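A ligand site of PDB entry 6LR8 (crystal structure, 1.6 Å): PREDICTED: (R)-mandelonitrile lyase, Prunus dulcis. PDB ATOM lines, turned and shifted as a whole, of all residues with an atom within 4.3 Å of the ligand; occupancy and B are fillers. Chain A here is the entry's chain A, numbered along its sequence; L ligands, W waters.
O1 of the ligand is in hydrogen-bond range of N of Thr 42 (3.0 Å).
A nitrogen (N5) of the ligand sits at hydrogen-bond distance from the backbone NH (N) of Arg 62 (3.1 Å).
N of Thr 112 is in hydrogen-bond range of O1 of the ligand, 2.8 Å away.
O of Val 223 sits at hydrogen-bond distance from N3 of the ligand (2.9 Å).
An oxygen (O13) of the ligand lies within hydrogen-bond range of the backbone NH (N) of Ser 43, 3.2 Å away.
The side-chain hydroxyl (OG1) of Thr 112 sits at hydrogen-bond distance from an oxygen (O2) of the ligand (2.7 Å).
An oxygen (O9) of the ligand lies within hydrogen-bond range of the side-chain amide nitrogen (ND2) of Asn 116, at 3.2 Å.
N of Ala 494 lies within hydrogen-bond range of O14 of the ligand, 2.9 Å away.
O8 of the ligand sits at hydrogen-bond distance from N of Gly 118 (3.1 Å).
The guanidinium group (NE) of Arg 62 lies within hydrogen-bond range of an oxygen (O6) of the ligand.
The backbone NH of Gln 506 lies within hydrogen-bond range of an oxygen (O7) of the ligand (2.8 Å).
N of Val 119 sits at hydrogen-bond distance from O8 of the ligand (2.9 Å).
The backbone carbonyl oxygen (O) of Val 119 lies within hydrogen-bond range of a nitrogen (N7) of the ligand, at 3.0 Å.
The side-chain hydroxyl (OG1) of Thr 42 sits at hydrogen-bond distance from an oxygen (O11) of the ligand (2.6 Å).
An oxygen (O6) of the ligand is in hydrogen-bond range of the side-chain carboxylate of Glu 61.
An oxygen (O5) of the ligand lies within hydrogen-bond range of the backbone carbonyl oxygen (O) of Ile 108, 3.1 Å away.
N of Val 223 sits at hydrogen-bond distance from N4 of the ligand (3.0 Å).
N of Ala 117 is in hydrogen-bond range of N8 of the ligand (3.0 Å).
O of Ala 106 sits at hydrogen-bond distance from O6 of the ligand (3.4 Å).
The backbone NH (N) of Ser 263 lies within hydrogen-bond range of the backbone carbonyl oxygen (O) of Ile 38 (2.7 Å).
N of Gly 265 is in hydrogen-bond range of OD2 of Asp 493.
NE2 of Gln 506 is in hydrogen-bond range of O of Val 119, 3.0 Å away.
The backbone NH of Ala 221 sits at hydrogen-bond distance from the backbone carbonyl oxygen of Glu 61 (2.9 Å).
OE1 of Glu 61 lies within hydrogen-bond range of N of Gly 40, 2.8 Å away.
The backbone NH (N) of Ile 108 sits at hydrogen-bond distance from the side-chain carboxylate (OE2) of Glu 61 (3.3 Å).
The backbone NH of Arg 62 lies close to the backbone carbonyl oxygen of Ala 221.
N of Ala 264 is in hydrogen-bond range of O of Ile 38.
An oxygen (O7) of the ligand sits close to the backbone carbonyl oxygen (O) of His 504, at 3.1 Å.
O7 of the ligand sits close to N of Pro 505 (2.9 Å).
Residues that only touch the ligand: Trp 465, Gly 111, Gly 41, Gly 39, Ala 221, Asp 493, Ser 263, His 466, Ala 264, Arg 107, Val 386, Gly 265, Val 104, Leu 60 and Gly 40.
Within 4 Å of the ligand: Gly 39, Gly 40, Gly 41, Thr 42, Ser 43, Leu 60, Glu 61, Arg 62, Val 104, Ala 106, Arg 107, Ile 108, Gly 111, Thr 112, Asn 116, Ala 117, Gly 118, Val 119, Ala 221, Val 223, Ser 263, Ala 264, Gly 265, Val 386, Trp 465, His 466, Asp 493, Ala 494, His 504, Pro 505 and Gln 506.
Along chain A the residues within 4 Å of the ligand span positions 39 to 506.
Water W6 bridges O2 of the ligand and O of Ala 106.
Water W3 bridges O10 of the ligand (2.9 Å) and O of His 466 (3.4 Å).
Water W10 bridges the backbone carbonyl oxygen (O) of Gly 268 and a nitrogen (N3) of the ligand.
Water W9 lies within hydrogen-bond range of NE2 of His 466 (2.8 Å) and N8 of the ligand (3.2 Å).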
ATOM      1  N   ILE A  38      -1.033  -6.568  31.206  1.00  0.00           N
ATOM      2  CA  ILE A  38      -1.556  -5.542  30.313  1.00  0.00           C
ATOM      3  C   ILE A  38      -1.285  -5.978  28.892  1.00  0.00           C
ATOM      4  O   ILE A  38      -0.133  -5.966  28.448  1.00  0.00           O
ATOM      5  CB  ILE A  38      -0.894  -4.190  30.589  1.00  0.00           C
ATOM      6  CG1 ILE A  38      -1.100  -3.773  32.049  1.00  0.00           C
ATOM      7  CG2 ILE A  38      -1.438  -3.147  29.616  1.00  0.00           C
ATOM      8  CD1 ILE A  38      -0.096  -2.727  32.489  1.00  0.00           C
ATOM      9  N   GLY A  39      -2.350  -6.329  28.161  1.00  0.00           N
ATOM     10  CA  GLY A  39      -2.204  -6.757  26.779  1.00  0.00           C
ATOM     11  C   GLY A  39      -2.418  -8.254  26.650  1.00  0.00           C
ATOM     12  O   GLY A  39      -1.550  -9.050  27.035  1.00  0.00           O
ATOM     13  N   GLY A  40      -3.560  -8.650  26.108  1.00  0.00           N
ATOM     14  CA  GLY A  40      -3.871 -10.060  25.972  1.00  0.00           C
ATOM     15  C   GLY A  40      -3.410 -10.575  24.634  1.00  0.00           C
ATOM     16  O   GLY A  40      -4.218 -10.999  23.812  1.00  0.00           O
ATOM     17  N   GLY A  41      -2.098 -10.527  24.395  1.00  0.00           N
ATOM     18  CA  GLY A  41      -1.563 -10.836  23.088  1.00  0.00           C
ATOM     19  C   GLY A  41      -0.696 -12.080  23.094  1.00  0.00           C
ATOM     20  O   GLY A  41      -0.922 -13.012  23.876  1.00  0.00           O
ATOM     21  N   THR A  42       0.303 -12.075  22.203  1.00  0.00           N
ATOM     22  CA  THR A  42       1.139 -13.247  21.959  1.00  0.00           C
ATOM     23  C   THR A  42       1.849 -13.709  23.229  1.00  0.00           C
ATOM     24  O   THR A  42       1.796 -14.888  23.577  1.00  0.00           O
ATOM     25  CB  THR A  42       2.143 -12.914  20.856  1.00  0.00           C
ATOM     26  OG1 THR A  42       1.433 -12.390  19.714  1.00  0.00           O
ATOM     27  CG2 THR A  42       2.962 -14.146  20.435  1.00  0.00           C
ATOM     28  N   SER A  43       2.510 -12.796  23.927  1.00  0.00           N
ATOM     29  CA  SER A  43       3.144 -13.130  25.196  1.00  0.00           C
ATOM     30  C   SER A  43       2.154 -13.055  26.348  1.00  0.00           C
ATOM     31  O   SER A  43       2.217 -13.870  27.283  1.00  0.00           O
ATOM     32  CB  SER A  43       4.334 -12.205  25.479  1.00  0.00           C
ATOM     33  OG  SER A  43       5.413 -12.433  24.576  1.00  0.00           O
ATOM     34  N   LEU A  60      -5.844  -7.650  31.010  1.00  0.00           N
ATOM     35  CA  LEU A  60      -6.561  -6.512  30.440  1.00  0.00           C
ATOM     36  C   LEU A  60      -6.201  -6.375  28.968  1.00  0.00           C
ATOM     37  O   LEU A  60      -5.028  -6.205  28.632  1.00  0.00           O
ATOM     38  CB  LEU A  60      -6.212  -5.226  31.179  1.00  0.00           C
ATOM     39  CG  LEU A  60      -6.575  -5.227  32.657  1.00  0.00           C
ATOM     40  CD1 LEU A  60      -6.001  -4.009  33.368  1.00  0.00           C
ATOM     41  CD2 LEU A  60      -8.081  -5.299  32.822  1.00  0.00           C
ATOM     42  N   GLU A  61      -7.212  -6.422  28.094  1.00  0.00           N
ATOM     43  CA  GLU A  61      -7.001  -6.317  26.656  1.00  0.00           C
ATOM     44  C   GLU A  61      -7.886  -5.234  26.054  1.00  0.00           C
ATOM     45  O   GLU A  61      -9.094  -5.212  26.301  1.00  0.00           O
ATOM     46  CB  GLU A  61      -7.273  -7.687  25.985  1.00  0.00           C
ATOM     47  CG  GLU A  61      -7.450  -7.625  24.458  1.00  0.00           C
ATOM     48  CD  GLU A  61      -6.230  -7.072  23.756  1.00  0.00           C
ATOM     49  OE1 GLU A  61      -5.090  -7.418  24.144  1.00  0.00           O
ATOM     50  OE2 GLU A  61      -6.411  -6.299  22.784  1.00  0.00           O
ATOM     51  N   ARG A  62      -7.301  -4.345  25.253  1.00  0.00           N
ATOM     52  CA  ARG A  62      -8.066  -3.230  24.707  1.00  0.00           C
ATOM     53  C   ARG A  62      -9.052  -3.649  23.618  1.00  0.00           C
ATOM     54  O   ARG A  62     -10.051  -2.949  23.406  1.00  0.00           O
ATOM     55  CB  ARG A  62      -7.117  -2.159  24.149  1.00  0.00           C
ATOM     56  CG  ARG A  62      -6.308  -2.643  22.976  1.00  0.00           C
ATOM     57  CD  ARG A  62      -5.358  -1.588  22.430  1.00  0.00           C
ATOM     58  NE  ARG A  62      -4.718  -2.104  21.221  1.00  0.00           N
ATOM     59  CZ  ARG A  62      -4.322  -1.362  20.198  1.00  0.00           C
ATOM     60  NH1 ARG A  62      -4.439  -0.029  20.251  1.00  0.00           N
ATOM     61  NH2 ARG A  62      -3.786  -1.947  19.127  1.00  0.00           N
ATOM     62  N   VAL A 104       0.571  -2.497  10.277  1.00  0.00           N
ATOM     63  CA  VAL A 104      -0.573  -2.855  11.102  1.00  0.00           C
ATOM     64  C   VAL A 104      -0.094  -3.440  12.422  1.00  0.00           C
ATOM     65  O   VAL A 104       1.022  -3.957  12.539  1.00  0.00           O
ATOM     66  CB  VAL A 104      -1.528  -3.874  10.428  1.00  0.00           C
ATOM     67  CG1 VAL A 104      -2.082  -3.348   9.100  1.00  0.00           C
ATOM     68  CG2 VAL A 104      -0.824  -5.205  10.228  1.00  0.00           C
ATOM     69  N   ALA A 106      -2.152  -5.545  16.042  1.00  0.00           N
ATOM     70  CA  ALA A 106      -3.390  -6.203  16.428  1.00  0.00           C
ATOM     71  C   ALA A 106      -4.116  -5.430  17.524  1.00  0.00           C
ATOM     72  O   ALA A 106      -3.512  -4.703  18.308  1.00  0.00           O
ATOM     73  CB  ALA A 106      -3.118  -7.617  16.942  1.00  0.00           C
ATOM     74  N   ARG A 107      -5.441  -5.621  17.570  1.00  0.00           N
ATOM     75  CA  ARG A 107      -6.297  -4.979  18.569  1.00  0.00           C
ATOM     76  C   ARG A 107      -7.412  -5.996  18.861  1.00  0.00           C
ATOM     77  O   ARG A 107      -8.549  -5.853  18.404  1.00  0.00           O
ATOM     78  CB  ARG A 107      -6.853  -3.651  18.075  1.00  0.00           C
ATOM     79  CG  ARG A 107      -7.671  -2.877  19.088  1.00  0.00           C
ATOM     80  CD  ARG A 107      -8.005  -1.458  18.569  1.00  0.00           C
ATOM     81  NE  ARG A 107      -8.478  -1.551  17.209  1.00  0.00           N
ATOM     82  CZ  ARG A 107      -8.366  -0.624  16.266  1.00  0.00           C
ATOM     83  NH1 ARG A 107      -7.800   0.565  16.486  1.00  0.00           N
ATOM     84  NH2 ARG A 107      -8.846  -0.913  15.065  1.00  0.00           N
ATOM     85  N   ILE A 108      -7.070  -7.041  19.613  1.00  0.00           N
ATOM     86  CA  ILE A 108      -7.979  -8.187  19.751  1.00  0.00           C
ATOM     87  C   ILE A 108      -7.411  -9.131  20.800  1.00  0.00           C
ATOM     88  O   ILE A 108      -6.189  -9.210  20.968  1.00  0.00           O
ATOM     89  CB  ILE A 108      -8.157  -8.907  18.390  1.00  0.00           C
ATOM     90  CG1 ILE A 108      -9.429  -9.759  18.364  1.00  0.00           C
ATOM     91  CG2 ILE A 108      -6.945  -9.765  18.065  1.00  0.00           C
ATOM     92  CD1 ILE A 108     -10.729  -8.940  18.279  1.00  0.00           C
ATOM     93  N   GLY A 111      -4.123 -11.025  20.467  1.00  0.00           N
ATOM     94  CA  GLY A 111      -3.085 -10.180  19.890  1.00  0.00           C
ATOM     95  C   GLY A 111      -2.784 -10.534  18.445  1.00  0.00           C
ATOM     96  O   GLY A 111      -3.664 -10.919  17.669  1.00  0.00           O
ATOM     97  N   THR A 112      -1.514 -10.402  18.082  1.00  0.00           N
ATOM     98  CA  THR A 112      -1.178 -10.504  16.667  1.00  0.00           C
ATOM     99  C   THR A 112      -1.280 -11.951  16.155  1.00  0.00           C
ATOM    100  O   THR A 112      -1.415 -12.160  14.940  1.00  0.00           O
ATOM    101  CB  THR A 112       0.184  -9.850  16.446  1.00  0.00           C
ATOM    102  OG1 THR A 112       0.079  -8.473  16.870  1.00  0.00           O
ATOM    103  CG2 THR A 112       0.598  -9.884  14.984  1.00  0.00           C
ATOM    104  N   THR A 113      -1.290 -12.942  17.051  1.00  0.00           N
ATOM    105  CA  THR A 113      -1.561 -14.312  16.612  1.00  0.00           C
ATOM    106  C   THR A 113      -2.952 -14.487  16.023  1.00  0.00           C
ATOM    107  O   THR A 113      -3.198 -15.508  15.366  1.00  0.00           O
ATOM    108  CB  THR A 113      -1.363 -15.316  17.776  1.00  0.00           C
ATOM    109  OG1 THR A 113      -2.382 -15.167  18.772  1.00  0.00           O
ATOM    110  CG2 THR A 113       0.033 -15.132  18.395  1.00  0.00           C
ATOM    111  N   ILE A 115      -4.250 -12.345  13.779  1.00  0.00           N
ATOM    112  CA  ILE A 115      -4.290 -11.693  12.475  1.00  0.00           C
ATOM    113  C   ILE A 115      -3.092 -12.043  11.598  1.00  0.00           C
ATOM    114  O   ILE A 115      -3.015 -11.560  10.462  1.00  0.00           O
ATOM    115  CB  ILE A 115      -4.399 -10.158  12.596  1.00  0.00           C
ATOM    116  CG1 ILE A 115      -3.149  -9.556  13.272  1.00  0.00           C
ATOM    117  CG2 ILE A 115      -5.675  -9.761  13.332  1.00  0.00           C
ATOM    118  CD1 ILE A 115      -3.031  -8.024  13.138  1.00  0.00           C
ATOM    119  N   ASN A 116      -2.173 -12.881  12.076  1.00  0.00           N
ATOM    120  CA  ASN A 116      -0.895 -13.010  11.414  1.00  0.00           C
ATOM    121  C   ASN A 116      -0.927 -14.113  10.351  1.00  0.00           C
ATOM    122  O   ASN A 116      -1.973 -14.683  10.046  1.00  0.00           O
ATOM    123  CB  ASN A 116       0.212 -13.176  12.466  1.00  0.00           C
ATOM    124  CG  ASN A 116       0.248 -14.526  13.147  1.00  0.00           C
ATOM    125  OD1 ASN A 116      -0.485 -15.451  12.812  1.00  0.00           O
ATOM    126  ND2 ASN A 116       1.127 -14.636  14.138  1.00  0.00           N
ATOM    127  N   ALA A 117       0.231 -14.381   9.742  1.00  0.00           N
ATOM    128  CA  ALA A 117       0.289 -15.305   8.615  1.00  0.00           C
ATOM    129  C   ALA A 117       0.488 -16.755   9.044  1.00  0.00           C
ATOM    130  O   ALA A 117       0.645 -17.628   8.183  1.00  0.00           O
ATOM    131  CB  ALA A 117       1.398 -14.861   7.652  1.00  0.00           C
ATOM    132  N   GLY A 118       0.484 -17.031  10.356  1.00  0.00           N
ATOM    133  CA  GLY A 118       0.425 -18.392  10.865  1.00  0.00           C
ATOM    134  C   GLY A 118       1.735 -19.143  10.926  1.00  0.00           C
ATOM    135  O   GLY A 118       1.733 -20.304  11.351  1.00  0.00           O
ATOM    136  N   VAL A 119       2.852 -18.560  10.490  1.00  0.00           N
ATOM    137  CA  VAL A 119       4.088 -19.326  10.390  1.00  0.00           C
ATOM    138  C   VAL A 119       4.654 -19.564  11.789  1.00  0.00           C
ATOM    139  O   VAL A 119       4.765 -18.628  12.599  1.00  0.00           O
ATOM    140  CB  VAL A 119       5.119 -18.603   9.507  1.00  0.00           C
ATOM    141  CG1 VAL A 119       6.386 -19.440   9.353  1.00  0.00           C
ATOM    142  CG2 VAL A 119       4.510 -18.289   8.136  1.00  0.00           C
ATOM    143  N   ALA A 221     -10.726  -3.154  27.455  1.00  0.00           N
ATOM    144  CA  ALA A 221     -10.086  -2.506  28.605  1.00  0.00           C
ATOM    145  C   ALA A 221      -8.866  -1.773  28.062  1.00  0.00           C
ATOM    146  O   ALA A 221      -7.844  -2.391  27.750  1.00  0.00           O
ATOM    147  CB  ALA A 221      -9.701  -3.533  29.667  1.00  0.00           C
ATOM    148  N   SER A 222      -8.976  -0.454  27.951  1.00  0.00           N
ATOM    149  CA  SER A 222      -7.881   0.370  27.428  1.00  0.00           C
ATOM    150  C   SER A 222      -7.051   0.838  28.619  1.00  0.00           C
ATOM    151  O   SER A 222      -7.485   1.713  29.378  1.00  0.00           O
ATOM    152  CB  SER A 222      -8.463   1.544  26.652  1.00  0.00           C
ATOM    153  OG  SER A 222      -7.477   2.482  26.252  1.00  0.00           O
ATOM    154  N   VAL A 223      -5.868   0.253  28.809  1.00  0.00           N
ATOM    155  CA  VAL A 223      -5.047   0.613  29.965  1.00  0.00           C
ATOM    156  C   VAL A 223      -4.325   1.918  29.665  1.00  0.00           C
ATOM    157  O   VAL A 223      -3.555   1.996  28.702  1.00  0.00           O
ATOM    158  CB  VAL A 223      -4.047  -0.502  30.314  1.00  0.00           C
ATOM    159  CG1 VAL A 223      -3.209  -0.062  31.499  1.00  0.00           C
ATOM    160  CG2 VAL A 223      -4.808  -1.792  30.622  1.00  0.00           C
ATOM    161  N   SER A 263       2.519  -6.236  28.569  1.00  0.00           N
ATOM    162  CA  SER A 263       2.627  -7.124  27.421  1.00  0.00           C
ATOM    163  C   SER A 263       1.885  -6.505  26.244  1.00  0.00           C
ATOM    164  O   SER A 263       1.214  -7.192  25.468  1.00  0.00           O
ATOM    165  CB  SER A 263       2.088  -8.514  27.761  1.00  0.00           C
ATOM    166  OG  SER A 263       2.891  -9.109  28.790  1.00  0.00           O
ATOM    167  N   ALA A 264       2.012  -5.187  26.095  1.00  0.00           N
ATOM    168  CA  ALA A 264       1.219  -4.414  25.151  1.00  0.00           C
ATOM    169  C   ALA A 264       1.885  -4.266  23.780  1.00  0.00           C
ATOM    170  O   ALA A 264       1.365  -3.537  22.930  1.00  0.00           O
ATOM    171  CB  ALA A 264       0.914  -3.032  25.739  1.00  0.00           C
ATOM    172  N   GLY A 265       2.984  -4.975  23.542  1.00  0.00           N
ATOM    173  CA  GLY A 265       3.622  -5.011  22.239  1.00  0.00           C
ATOM    174  C   GLY A 265       4.694  -3.955  22.062  1.00  0.00           C
ATOM    175  O   GLY A 265       4.875  -3.039  22.874  1.00  0.00           O
ATOM    176  N   GLY A 268       2.681  -0.686  21.979  1.00  0.00           N
ATOM    177  CA  GLY A 268       1.896  -0.347  23.149  1.00  0.00           C
ATOM    178  C   GLY A 268       2.683  -0.270  24.443  1.00  0.00           C
ATOM    179  O   GLY A 268       2.343   0.532  25.321  1.00  0.00           O
ATOM    180  N   VAL A 386      -4.158   7.186  25.415  1.00  0.00           N
ATOM    181  CA  VAL A 386      -3.525   5.950  24.967  1.00  0.00           C
ATOM    182  C   VAL A 386      -4.186   5.396  23.708  1.00  0.00           C
ATOM    183  O   VAL A 386      -3.588   4.560  23.029  1.00  0.00           O
ATOM    184  CB  VAL A 386      -3.544   4.907  26.107  1.00  0.00           C
ATOM    185  CG1 VAL A 386      -4.922   4.246  26.213  1.00  0.00           C
ATOM    186  CG2 VAL A 386      -2.482   3.842  25.862  1.00  0.00           C
ATOM    187  N   TRP A 465       6.415  -6.881   9.247  1.00  0.00           N
ATOM    188  CA  TRP A 465       5.449  -6.938  10.327  1.00  0.00           C
ATOM    189  C   TRP A 465       6.072  -7.529  11.590  1.00  0.00           C
ATOM    190  O   TRP A 465       5.365  -7.715  12.604  1.00  0.00           O
ATOM    191  CB  TRP A 465       4.203  -7.751   9.964  1.00  0.00           C
ATOM    192  CG  TRP A 465       3.397  -7.260   8.799  1.00  0.00           C
ATOM    193  CD1 TRP A 465       2.957  -5.983   8.577  1.00  0.00           C
ATOM    194  CD2 TRP A 465       2.880  -8.043   7.709  1.00  0.00           C
ATOM    195  NE1 TRP A 465       2.222  -5.928   7.404  1.00  0.00           N
ATOM    196  CE2 TRP A 465       2.155  -7.177   6.861  1.00  0.00           C
ATOM    197  CE3 TRP A 465       2.958  -9.398   7.373  1.00  0.00           C
ATOM    198  CZ2 TRP A 465       1.531  -7.629   5.698  1.00  0.00           C
ATOM    199  CZ3 TRP A 465       2.326  -9.844   6.219  1.00  0.00           C
ATOM    200  CH2 TRP A 465       1.623  -8.954   5.388  1.00  0.00           C
ATOM    201  N   HIS A 466       7.372  -7.820  11.583  1.00  0.00           N
ATOM    202  CA  HIS A 466       8.036  -8.461  12.715  1.00  0.00           C
ATOM    203  C   HIS A 466       8.808  -7.449  13.534  1.00  0.00           C
ATOM    204  O   HIS A 466       9.945  -7.715  13.953  1.00  0.00           O
ATOM    205  CB  HIS A 466       8.951  -9.569  12.219  1.00  0.00           C
ATOM    206  CG  HIS A 466       8.231 -10.679  11.519  1.00  0.00           C
ATOM    207  ND1 HIS A 466       8.888 -11.807  11.066  1.00  0.00           N
ATOM    208  CD2 HIS A 466       6.926 -10.853  11.195  1.00  0.00           C
ATOM    209  CE1 HIS A 466       8.027 -12.621  10.494  1.00  0.00           C
ATOM    210  NE2 HIS A 466       6.835 -12.057  10.540  1.00  0.00           N
ATOM    211  N   ASP A 493       7.061  -9.157  25.991  1.00  0.00           N
ATOM    212  CA  ASP A 493       6.484  -9.093  24.639  1.00  0.00           C
ATOM    213  C   ASP A 493       7.616  -8.778  23.662  1.00  0.00           C
ATOM    214  O   ASP A 493       8.798  -8.823  24.046  1.00  0.00           O
ATOM    215  CB  ASP A 493       5.356  -8.056  24.561  1.00  0.00           C
ATOM    216  CG  ASP A 493       5.793  -6.660  24.954  1.00  0.00           C
ATOM    217  OD1 ASP A 493       6.994  -6.356  24.852  1.00  0.00           O
ATOM    218  OD2 ASP A 493       4.933  -5.863  25.360  1.00  0.00           O
ATOM    219  N   ALA A 494       7.297  -8.441  22.411  1.00  0.00           N
ATOM    220  CA  ALA A 494       8.377  -8.226  21.450  1.00  0.00           C
ATOM    221  C   ALA A 494       9.116  -6.906  21.637  1.00  0.00           C
ATOM    222  O   ALA A 494      10.078  -6.647  20.910  1.00  0.00           O
ATOM    223  CB  ALA A 494       7.823  -8.322  20.020  1.00  0.00           C
ATOM    224  N   HIS A 504      10.463 -15.869  12.031  1.00  0.00           N
ATOM    225  CA  HIS A 504       9.042 -15.760  12.315  1.00  0.00           C
ATOM    226  C   HIS A 504       8.919 -15.899  13.822  1.00  0.00           C
ATOM    227  O   HIS A 504       8.975 -17.020  14.356  1.00  0.00           O
ATOM    228  CB  HIS A 504       8.238 -16.828  11.576  1.00  0.00           C
ATOM    229  CG  HIS A 504       8.196 -16.604  10.100  1.00  0.00           C
ATOM    230  ND1 HIS A 504       9.205 -17.013   9.258  1.00  0.00           N
ATOM    231  CD2 HIS A 504       7.290 -15.950   9.329  1.00  0.00           C
ATOM    232  CE1 HIS A 504       8.920 -16.646   8.030  1.00  0.00           C
ATOM    233  NE2 HIS A 504       7.767 -15.999   8.037  1.00  0.00           N
ATOM    234  N   PRO A 505       8.752 -14.788  14.535  1.00  0.00           N
ATOM    235  CA  PRO A 505       8.992 -14.767  15.983  1.00  0.00           C
ATOM    236  C   PRO A 505       7.816 -15.121  16.871  1.00  0.00           C
ATOM    237  O   PRO A 505       8.003 -15.125  18.088  1.00  0.00           O
ATOM    238  CB  PRO A 505       9.398 -13.300  16.198  1.00  0.00           C
ATOM    239  CG  PRO A 505       8.555 -12.555  15.197  1.00  0.00           C
ATOM    240  CD  PRO A 505       8.580 -13.443  13.965  1.00  0.00           C
ATOM    241  N   GLN A 506       6.610 -15.392  16.341  1.00  0.00           N
ATOM    242  CA  GLN A 506       5.488 -15.656  17.233  1.00  0.00           C
ATOM    243  C   GLN A 506       5.775 -16.850  18.144  1.00  0.00           C
ATOM    244  O   GLN A 506       5.466 -16.809  19.340  1.00  0.00           O
ATOM    245  CB  GLN A 506       4.171 -15.845  16.457  1.00  0.00           C
ATOM    246  CG  GLN A 506       3.969 -17.195  15.773  1.00  0.00           C
ATOM    247  CD  GLN A 506       2.511 -17.455  15.387  1.00  0.00           C
ATOM    248  OE1 GLN A 506       1.588 -16.938  16.008  1.00  0.00           O
ATOM    249  NE2 GLN A 506       2.303 -18.261  14.347  1.00  0.00           N
HETATM  250  P1  LIG L   1       0.704  -8.495  20.395  1.00  0.00           P
HETATM  251  O1  LIG L   1       0.431  -9.921  20.105  1.00  0.00           O
HETATM  252  O2  LIG L   1       0.241  -7.497  19.366  1.00  0.00           O
HETATM  253  O3  LIG L   1       0.031  -8.225  21.814  1.00  0.00           O
HETATM  254  C1  LIG L   1      -0.133  -6.892  22.338  1.00  0.00           C
HETATM  255  C2  LIG L   1      -1.557  -6.800  22.830  1.00  0.00           C
HETATM  256  O4  LIG L   1      -1.672  -5.649  23.689  1.00  0.00           O
HETATM  257  C3  LIG L   1      -2.600  -6.629  21.727  1.00  0.00           C
HETATM  258  O5  LIG L   1      -3.627  -7.618  21.838  1.00  0.00           O
HETATM  259  C4  LIG L   1      -3.098  -5.196  21.921  1.00  0.00           C
HETATM  260  O6  LIG L   1      -4.464  -5.018  21.551  1.00  0.00           O
HETATM  261  C5  LIG L   1      -2.905  -5.015  23.414  1.00  0.00           C
HETATM  262  N1  LIG L   1      -2.791  -3.649  23.894  1.00  0.00           N
HETATM  263  C6  LIG L   1      -1.923  -2.684  23.435  1.00  0.00           C
HETATM  264  N2  LIG L   1      -1.953  -1.563  24.117  1.00  0.00           N
HETATM  265  C7  LIG L   1      -2.866  -1.821  25.129  1.00  0.00           C
HETATM  266  C8  LIG L   1      -3.343  -1.044  26.193  1.00  0.00           C
HETATM  267  N3  LIG L   1      -2.952   0.216  26.442  1.00  0.00           N
HETATM  268  N4  LIG L   1      -4.265  -1.603  27.008  1.00  0.00           N
HETATM  269  C9  LIG L   1      -4.664  -2.852  26.777  1.00  0.00           C
HETATM  270  N5  LIG L   1      -4.278  -3.690  25.806  1.00  0.00           N
HETATM  271  C10 LIG L   1      -3.371  -3.106  25.013  1.00  0.00           C
HETATM  272  N6  LIG L   1       5.132 -13.837  13.257  1.00  0.00           N
HETATM  273  C11 LIG L   1       5.368 -15.146  12.961  1.00  0.00           C
HETATM  274  O7  LIG L   1       6.149 -15.832  13.640  1.00  0.00           O
HETATM  275  N7  LIG L   1       4.722 -15.746  11.901  1.00  0.00           N
HETATM  276  C12 LIG L   1       3.822 -15.117  11.037  1.00  0.00           C
HETATM  277  O8  LIG L   1       3.314 -15.743  10.107  1.00  0.00           O
HETATM  278  C13 LIG L   1       3.562 -13.732  11.358  1.00  0.00           C
HETATM  279  N8  LIG L   1       2.737 -13.061  10.587  1.00  0.00           N
HETATM  280  C14 LIG L   1       2.467 -11.736  10.927  1.00  0.00           C
HETATM  281  C15 LIG L   1       1.542 -11.036  10.153  1.00  0.00           C
HETATM  282  C16 LIG L   1       1.218  -9.718  10.469  1.00  0.00           C
HETATM  283  C17 LIG L   1       0.220  -8.988   9.601  1.00  0.00           C
HETATM  284  C18 LIG L   1       1.820  -9.094  11.568  1.00  0.00           C
HETATM  285  C19 LIG L   1       1.514  -7.651  11.907  1.00  0.00           C
HETATM  286  C20 LIG L   1       2.745  -9.793  12.342  1.00  0.00           C
HETATM  287  C21 LIG L   1       3.059 -11.120  12.033  1.00  0.00           C
HETATM  288  N9  LIG L   1       3.981 -11.861  12.799  1.00  0.00           N
HETATM  289  C22 LIG L   1       4.256 -13.178  12.490  1.00  0.00           C
HETATM  290  C23 LIG L   1       4.697 -11.242  13.919  1.00  0.00           C
HETATM  291  C24 LIG L   1       4.255 -11.754  15.270  1.00  0.00           C
HETATM  292  O9  LIG L   1       2.917 -12.219  15.162  1.00  0.00           O
HETATM  293  C25 LIG L   1       4.371 -10.603  16.274  1.00  0.00           C
HETATM  294  O10 LIG L   1       5.694 -10.092  16.255  1.00  0.00           O
HETATM  295  C26 LIG L   1       4.023 -11.027  17.695  1.00  0.00           C
HETATM  296  O11 LIG L   1       2.737 -11.651  17.651  1.00  0.00           O
HETATM  297  C27 LIG L   1       3.967  -9.825  18.608  1.00  0.00           C
HETATM  298  O12 LIG L   1       3.585 -10.257  19.931  1.00  0.00           O
HETATM  299  P2  LIG L   1       3.416  -9.225  21.100  1.00  0.00           P
HETATM  300  O13 LIG L   1       2.924 -10.006  22.324  1.00  0.00           O
HETATM  301  O14 LIG L   1       4.673  -8.424  21.249  1.00  0.00           O
HETATM  302  O15 LIG L   1       2.257  -8.257  20.598  1.00  0.00           O
HETATM  303  O   HOH W   1       1.136  -9.819  24.473  1.00  0.00           O
HETATM  304  O   HOH W   2       2.372  -5.909  18.271  1.00  0.00           O
HETATM  305  O   HOH W   3       8.540  -9.464  16.477  1.00  0.00           O
HETATM  306  O   HOH W   4       4.812  -6.425  19.279  1.00  0.00           O
HETATM  307  O   HOH W   5       6.850 -18.454  14.856  1.00  0.00           O
HETATM  308  O   HOH W   6      -0.858  -4.964  19.106  1.00  0.00           O
HETATM  309  O   HOH W   7       5.767  -7.369  16.819  1.00  0.00           O
HETATM  310  O   HOH W   8      -1.624   0.874  22.660  1.00  0.00           O
HETATM  311  O   HOH W   9       5.125 -12.837   8.413  1.00  0.00           O
HETATM  312  O   HOH W  10      -0.326   1.338  25.352  1.00  0.00           O
